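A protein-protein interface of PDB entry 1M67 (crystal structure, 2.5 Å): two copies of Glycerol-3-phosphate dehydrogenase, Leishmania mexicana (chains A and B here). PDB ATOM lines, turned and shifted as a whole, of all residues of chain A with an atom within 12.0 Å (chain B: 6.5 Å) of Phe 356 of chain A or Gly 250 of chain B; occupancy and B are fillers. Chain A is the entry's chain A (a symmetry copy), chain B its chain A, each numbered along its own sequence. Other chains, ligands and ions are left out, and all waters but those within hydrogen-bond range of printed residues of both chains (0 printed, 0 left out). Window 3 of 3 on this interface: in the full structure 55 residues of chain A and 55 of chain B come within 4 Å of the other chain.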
ATOM      1  N   PHE A 256      26.811 -22.455  15.843  1.00  0.00           N
ATOM      2  CA  PHE A 256      25.515 -21.945  16.234  1.00  0.00           C
ATOM      3  C   PHE A 256      25.482 -20.444  16.268  1.00  0.00           C
ATOM      4  O   PHE A 256      24.573 -19.886  16.818  1.00  0.00           O
ATOM      5  CB  PHE A 256      25.032 -22.544  17.541  1.00  0.00           C
ATOM      6  CG  PHE A 256      24.751 -24.005  17.447  1.00  0.00           C
ATOM      7  CD1 PHE A 256      25.470 -24.918  18.206  1.00  0.00           C
ATOM      8  CD2 PHE A 256      23.782 -24.468  16.573  1.00  0.00           C
ATOM      9  CE1 PHE A 256      25.213 -26.269  18.105  1.00  0.00           C
ATOM     10  CE2 PHE A 256      23.522 -25.816  16.471  1.00  0.00           C
ATOM     11  CZ  PHE A 256      24.235 -26.720  17.232  1.00  0.00           C
ATOM     12  N   LEU A 352      20.902 -33.937  20.231  1.00  0.00           N
ATOM     13  CA  LEU A 352      21.761 -32.833  20.629  1.00  0.00           C
ATOM     14  C   LEU A 352      22.232 -33.052  22.072  1.00  0.00           C
ATOM     15  O   LEU A 352      21.491 -33.544  22.921  1.00  0.00           O
ATOM     16  CB  LEU A 352      21.057 -31.479  20.464  1.00  0.00           C
ATOM     17  CG  LEU A 352      20.912 -30.941  19.037  1.00  0.00           C
ATOM     18  CD1 LEU A 352      20.025 -29.696  18.986  1.00  0.00           C
ATOM     19  CD2 LEU A 352      22.280 -30.637  18.442  1.00  0.00           C
ATOM     20  N   PRO A 353      23.483 -32.742  22.339  1.00  0.00           N
ATOM     21  CA  PRO A 353      24.000 -32.831  23.709  1.00  0.00           C
ATOM     22  C   PRO A 353      23.421 -31.744  24.603  1.00  0.00           C
ATOM     23  O   PRO A 353      23.004 -30.682  24.135  1.00  0.00           O
ATOM     24  CB  PRO A 353      25.491 -32.559  23.529  1.00  0.00           C
ATOM     25  CG  PRO A 353      25.531 -31.710  22.324  1.00  0.00           C
ATOM     26  CD  PRO A 353      24.528 -32.352  21.377  1.00  0.00           C
ATOM     27  N   PRO A 354      23.392 -32.023  25.895  1.00  0.00           N
ATOM     28  CA  PRO A 354      22.993 -31.028  26.887  1.00  0.00           C
ATOM     29  C   PRO A 354      24.009 -29.908  26.876  1.00  0.00           C
ATOM     30  O   PRO A 354      25.182 -30.165  26.616  1.00  0.00           O
ATOM     31  CB  PRO A 354      23.132 -31.778  28.214  1.00  0.00           C
ATOM     32  CG  PRO A 354      23.086 -33.205  27.855  1.00  0.00           C
ATOM     33  CD  PRO A 354      23.723 -33.322  26.500  1.00  0.00           C
ATOM     34  N   LEU A 355      23.572 -28.686  27.137  1.00  0.00           N
ATOM     35  CA  LEU A 355      24.512 -27.596  27.262  1.00  0.00           C
ATOM     36  C   LEU A 355      24.907 -27.502  28.733  1.00  0.00           C
ATOM     37  O   LEU A 355      26.050 -27.213  29.066  1.00  0.00           O
ATOM     38  CB  LEU A 355      23.877 -26.280  26.821  1.00  0.00           C
ATOM     39  CG  LEU A 355      23.255 -26.150  25.432  1.00  0.00           C
ATOM     40  CD1 LEU A 355      22.691 -24.753  25.283  1.00  0.00           C
ATOM     41  CD2 LEU A 355      24.275 -26.426  24.354  1.00  0.00           C
ATOM     42  N   PHE A 356      23.941 -27.767  29.607  1.00  0.00           N
ATOM     43  CA  PHE A 356      24.137 -27.647  31.041  1.00  0.00           C
ATOM     44  C   PHE A 356      23.946 -28.983  31.737  1.00  0.00           C
ATOM     45  O   PHE A 356      22.942 -29.667  31.547  1.00  0.00           O
ATOM     46  CB  PHE A 356      23.191 -26.592  31.594  1.00  0.00           C
ATOM     47  CG  PHE A 356      23.000 -25.432  30.658  1.00  0.00           C
ATOM     48  CD1 PHE A 356      24.049 -24.555  30.399  1.00  0.00           C
ATOM     49  CD2 PHE A 356      21.795 -25.247  29.999  1.00  0.00           C
ATOM     50  CE1 PHE A 356      23.888 -23.511  29.507  1.00  0.00           C
ATOM     51  CE2 PHE A 356      21.626 -24.205  29.114  1.00  0.00           C
ATOM     52  CZ  PHE A 356      22.669 -23.335  28.864  1.00  0.00           C
ATOM     53  N   LYS A 357      24.937 -29.341  32.544  1.00  0.00           N
ATOM     54  CA  LYS A 357      24.948 -30.601  33.260  1.00  0.00           C
ATOM     55  C   LYS A 357      24.155 -30.489  34.557  1.00  0.00           C
ATOM     56  O   LYS A 357      24.395 -29.587  35.358  1.00  0.00           O
ATOM     57  CB  LYS A 357      26.396 -31.016  33.545  1.00  0.00           C
ATOM     58  CG  LYS A 357      27.181 -31.444  32.297  1.00  0.00           C
ATOM     59  CD  LYS A 357      27.473 -30.275  31.341  1.00  0.00           C
ATOM     60  CE  LYS A 357      27.737 -30.779  29.910  1.00  0.00           C
ATOM     61  NZ  LYS A 357      28.013 -29.678  28.934  1.00  0.00           N
ATOM     62  N   ASP B 199      14.680 -32.232  27.191  1.00  0.00           N
ATOM     63  CA  ASP B 199      14.728 -30.838  27.611  1.00  0.00           C
ATOM     64  C   ASP B 199      13.382 -30.154  27.703  1.00  0.00           C
ATOM     65  O   ASP B 199      13.095 -29.242  26.909  1.00  0.00           O
ATOM     66  CB  ASP B 199      15.614 -30.051  26.650  1.00  0.00           C
ATOM     67  CG  ASP B 199      16.078 -28.742  27.236  1.00  0.00           C
ATOM     68  OD1 ASP B 199      16.769 -27.991  26.515  1.00  0.00           O
ATOM     69  OD2 ASP B 199      15.790 -28.396  28.401  1.00  0.00           O
ATOM     70  N   VAL B 201      12.299 -28.013  29.802  1.00  0.00           N
ATOM     71  CA  VAL B 201      12.461 -26.605  30.138  1.00  0.00           C
ATOM     72  C   VAL B 201      12.902 -25.759  28.953  1.00  0.00           C
ATOM     73  O   VAL B 201      12.334 -24.705  28.678  1.00  0.00           O
ATOM     74  CB  VAL B 201      13.503 -26.415  31.280  1.00  0.00           C
ATOM     75  CG1 VAL B 201      13.864 -24.952  31.411  1.00  0.00           C
ATOM     76  CG2 VAL B 201      12.975 -26.976  32.600  1.00  0.00           C
ATOM     77  N   GLY B 202      13.958 -26.197  28.278  1.00  0.00           N
ATOM     78  CA  GLY B 202      14.406 -25.488  27.094  1.00  0.00           C
ATOM     79  C   GLY B 202      13.220 -25.356  26.142  1.00  0.00           C
ATOM     80  O   GLY B 202      12.945 -24.265  25.634  1.00  0.00           O
ATOM     81  N   ILE B 241      17.442 -17.273  24.918  1.00  0.00           N
ATOM     82  CA  ILE B 241      16.693 -18.482  25.223  1.00  0.00           C
ATOM     83  C   ILE B 241      17.606 -19.484  25.940  1.00  0.00           C
ATOM     84  O   ILE B 241      17.183 -20.151  26.887  1.00  0.00           O
ATOM     85  CB  ILE B 241      16.111 -19.135  23.921  1.00  0.00           C
ATOM     86  CG1 ILE B 241      14.938 -18.332  23.408  1.00  0.00           C
ATOM     87  CG2 ILE B 241      15.635 -20.583  24.172  1.00  0.00           C
ATOM     88  CD1 ILE B 241      14.516 -18.789  22.053  1.00  0.00           C
ATOM     89  N   ARG B 242      18.843 -19.612  25.477  1.00  0.00           N
ATOM     90  CA  ARG B 242      19.793 -20.522  26.136  1.00  0.00           C
ATOM     91  C   ARG B 242      20.140 -20.110  27.605  1.00  0.00           C
ATOM     92  O   ARG B 242      20.259 -20.966  28.504  1.00  0.00           O
ATOM     93  CB  ARG B 242      21.094 -20.621  25.329  1.00  0.00           C
ATOM     94  CG  ARG B 242      22.270 -21.186  26.121  1.00  0.00           C
ATOM     95  CD  ARG B 242      23.640 -20.845  25.555  1.00  0.00           C
ATOM     96  NE  ARG B 242      23.985 -19.439  25.746  1.00  0.00           N
ATOM     97  CZ  ARG B 242      25.127 -18.892  25.363  1.00  0.00           C
ATOM     98  NH1 ARG B 242      26.061 -19.627  24.775  1.00  0.00           N
ATOM     99  NH2 ARG B 242      25.343 -17.608  25.556  1.00  0.00           N
ATOM    100  N   ASP B 243      20.285 -18.807  27.848  1.00  0.00           N
ATOM    101  CA  ASP B 243      20.700 -18.361  29.176  1.00  0.00           C
ATOM    102  C   ASP B 243      19.553 -18.448  30.181  1.00  0.00           C
ATOM    103  O   ASP B 243      19.768 -18.695  31.377  1.00  0.00           O
ATOM    104  CB  ASP B 243      21.250 -16.928  29.133  1.00  0.00           C
ATOM    105  CG  ASP B 243      22.533 -16.814  28.326  1.00  0.00           C
ATOM    106  OD1 ASP B 243      23.269 -17.817  28.199  1.00  0.00           O
ATOM    107  OD2 ASP B 243      22.887 -15.752  27.781  1.00  0.00           O
ATOM    108  N   LEU B 244      18.337 -18.205  29.702  1.00  0.00           N
ATOM    109  CA  LEU B 244      17.205 -18.243  30.591  1.00  0.00           C
ATOM    110  C   LEU B 244      16.990 -19.703  30.913  1.00  0.00           C
ATOM    111  O   LEU B 244      16.680 -20.073  32.009  1.00  0.00           O
ATOM    112  CB  LEU B 244      15.979 -17.635  29.922  1.00  0.00           C
ATOM    113  CG  LEU B 244      14.723 -17.668  30.773  1.00  0.00           C
ATOM    114  CD1 LEU B 244      15.061 -17.096  32.136  1.00  0.00           C
ATOM    115  CD2 LEU B 244      13.577 -16.923  30.124  1.00  0.00           C
ATOM    116  N   THR B 245      17.205 -20.541  29.932  1.00  0.00           N
ATOM    117  CA  THR B 245      17.080 -21.974  30.106  1.00  0.00           C
ATOM    118  C   THR B 245      18.056 -22.511  31.142  1.00  0.00           C
ATOM    119  O   THR B 245      17.671 -23.312  31.990  1.00  0.00           O
ATOM    120  CB  THR B 245      17.261 -22.653  28.726  1.00  0.00           C
ATOM    121  OG1 THR B 245      16.064 -22.446  27.969  1.00  0.00           O
ATOM    122  CG2 THR B 245      17.382 -24.172  28.848  1.00  0.00           C
ATOM    123  N   ALA B 246      19.311 -22.087  31.073  1.00  0.00           N
ATOM    124  CA  ALA B 246      20.320 -22.522  32.061  1.00  0.00           C
ATOM    125  C   ALA B 246      19.886 -22.206  33.505  1.00  0.00           C
ATOM    126  O   ALA B 246      19.925 -23.069  34.373  1.00  0.00           O
ATOM    127  CB  ALA B 246      21.695 -21.888  31.758  1.00  0.00           C
ATOM    128  N   ALA B 247      19.432 -20.970  33.712  1.00  0.00           N
ATOM    129  CA  ALA B 247      19.010 -20.438  35.010  1.00  0.00           C
ATOM    130  C   ALA B 247      17.813 -21.149  35.613  1.00  0.00           C
ATOM    131  O   ALA B 247      17.632 -21.157  36.845  1.00  0.00           O
ATOM    132  CB  ALA B 247      18.682 -18.950  34.871  1.00  0.00           C
ATOM    133  N   LEU B 248      16.977 -21.726  34.752  1.00  0.00           N
ATOM    134  CA  LEU B 248      15.774 -22.393  35.233  1.00  0.00           C
ATOM    135  C   LEU B 248      15.984 -23.876  35.458  1.00  0.00           C
ATOM    136  O   LEU B 248      15.031 -24.573  35.809  1.00  0.00           O
ATOM    137  CB  LEU B 248      14.624 -22.191  34.263  1.00  0.00           C
ATOM    138  CG  LEU B 248      14.100 -20.780  34.084  1.00  0.00           C
ATOM    139  CD1 LEU B 248      13.584 -20.621  32.682  1.00  0.00           C
ATOM    140  CD2 LEU B 248      13.007 -20.434  35.100  1.00  0.00           C
ATOM    141  N   GLY B 249      17.194 -24.373  35.207  1.00  0.00           N
ATOM    142  CA  GLY B 249      17.490 -25.772  35.459  1.00  0.00           C
ATOM    143  C   GLY B 249      17.525 -26.719  34.271  1.00  0.00           C
ATOM    144  O   GLY B 249      17.888 -27.885  34.419  1.00  0.00           O
ATOM    145  N   GLY B 250      17.170 -26.240  33.088  1.00  0.00           N
ATOM    146  CA  GLY B 250      17.132 -27.092  31.918  1.00  0.00           C
ATOM    147  C   GLY B 250      18.496 -27.526  31.445  1.00  0.00           C
ATOM    148  O   GLY B 250      19.491 -26.854  31.680  1.00  0.00           O
ATOM    149  N   ASP B 251      18.552 -28.659  30.765  1.00  0.00           N
ATOM    150  CA  ASP B 251      19.834 -29.153  30.285  1.00  0.00           C
ATOM    151  C   ASP B 251      20.215 -28.489  28.968  1.00  0.00           C
ATOM    152  O   ASP B 251      21.347 -28.633  28.491  1.00  0.00           O
ATOM    153  CB  ASP B 251      19.814 -30.673  30.140  1.00  0.00           C
ATOM    154  CG  ASP B 251      18.993 -31.122  28.967  1.00  0.00           C
ATOM    155  OD1 ASP B 251      18.024 -31.881  29.174  1.00  0.00           O
ATOM    156  OD2 ASP B 251      19.229 -30.758  27.799  1.00  0.00           O
ATOM    157  N   GLY B 252      19.270 -27.767  28.373  1.00  0.00           N
ATOM    158  CA  GLY B 252      19.556 -27.009  27.161  1.00  0.00           C
ATOM    159  C   GLY B 252      19.660 -27.714  25.811  1.00  0.00           C
ATOM    160  O   GLY B 252      19.912 -27.065  24.812  1.00  0.00           O
ATOM    161  N   SER B 253      19.479 -29.027  25.762  1.00  0.00           N
ATOM    162  CA  SER B 253      19.592 -29.750  24.491  1.00  0.00           C
ATOM    163  C   SER B 253      18.495 -29.437  23.457  1.00  0.00           C
ATOM    164  O   SER B 253      18.643 -29.778  22.286  1.00  0.00           O
ATOM    165  CB  SER B 253      19.686 -31.260  24.704  1.00  0.00           C
ATOM    166  OG  SER B 253      18.512 -31.761  25.309  1.00  0.00           O
ATOM    167  N   VAL B 255      17.546 -26.350  22.842  1.00  0.00           N
ATOM    168  CA  VAL B 255      17.864 -25.000  22.392  1.00  0.00           C
ATOM    169  C   VAL B 255      18.285 -24.868  20.936  1.00  0.00           C
ATOM    170  O   VAL B 255      17.765 -24.024  20.206  1.00  0.00           O
ATOM    171  CB  VAL B 255      18.958 -24.348  23.292  1.00  0.00           C
ATOM    172  CG1 VAL B 255      19.351 -22.989  22.754  1.00  0.00           C
ATOM    173  CG2 VAL B 255      18.459 -24.254  24.727  1.00  0.00           C
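No position is printed for both chains.
Of the 12 pairs that touch across the chains among the printed residues, none has its exchanged pair printed and touching as well.
OD1 of Asp 199 of chain B lies close to N of Gly 252 of chain B (3.1 Å).
N of Ser 253 of chain B sits at hydrogen-bond distance from OD1 of Asp 199 of chain B, at 3.0 Å.
The guanidinium group (NE) of Arg 242 of chain B is in salt-bridge range of the side-chain carboxylate (OD1) of Asp 243 of chain B (3.0 Å).
O of Thr 245 of chain B sits at hydrogen-bond distance from N of Gly 250 of chain B (3.2 Å).
OD2 of Asp 251 of chain B lies within hydrogen-bond range of N of Ser 253 of chain B.
O of Leu 355 of chain A is in hydrogen-bond range of NZ of Lys 357 of chain A (3.2 Å).
Printed residues of chain A that touch a printed residue of chain B: Leu 352, Pro 353, Pro 354, Leu 355 and Phe 356.
Hydrophobic or aromatic side chains of chain A that line the printed part of chain B: Leu 352, Pro 354, Leu 355 and Phe 356.
Hydrophobic or aromatic side chains of chain B within 4 Å of the printed part of chain A: Ala 246.
Of the printed residues of chain B, Leu 352 of chain A touches Ser 253 (3.4 Å).
Of the printed residues of chain B, Pro 353 of chain A touches Ser 253.
Of the printed residues of chain B, Leu 355 of chain A touches Arg 242 (3.7 Å), Asp 251 (2.6 Å) and Gly 252 (3.5 Å).
Lys 357 of chain A touches none of the printed residues of chain B.
No residue of chain A comes within 4 Å of Val 201 of chain B.
Leu 244 of chain B touches none of the printed residues of chain A.
No residue of chain A comes within 4 Å of Thr 245 of chain B.
Ala 246 of chain B touches one residue of chain A.
No residue of chain A comes within 4 Å of Leu 248 of chain B.
No residue of chain A comes within 4 Å of Gly 249 of chain B.
Gly 250 of chain B touches just one residue of chain A: Phe 356.
Asp 251 of chain B touches three residues of chain A.
The nearest printed residue of chain B that does not touch Leu 352 of chain A is Val 255 of chain B (5.5 Å).
Among the printed residues, pairs that only touch across the chains: Phe 356 of chain A with Gly 250 of chain B, Pro 354 of chain A with Asp 251 of chain B, Phe 356 of chain A with Ala 246 of chain B, Phe 356 of chain A with Arg 242 of chain B, Leu 352 of chain A with Ser 253 of chain B, Pro 353 of chain A with Ser 253 of chain B, Leu 355 of chain A with Gly 252 of chain B, Leu 355 of chain A with Arg 242 of chain B, Phe 356 of chain A with Gly 252 of chain B and Pro 354 of chain A with Ser 253 of chain B.
N of Leu 355 of chain A sits at hydrogen-bond distance from O of Asp 251 of chain B, at 2.6 Å.
The backbone carbonyl oxygen (O) of Asp 251 of chain B sits at hydrogen-bond distance from the backbone NH (N) of Phe 356 of chain A, at 3.0 Å.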
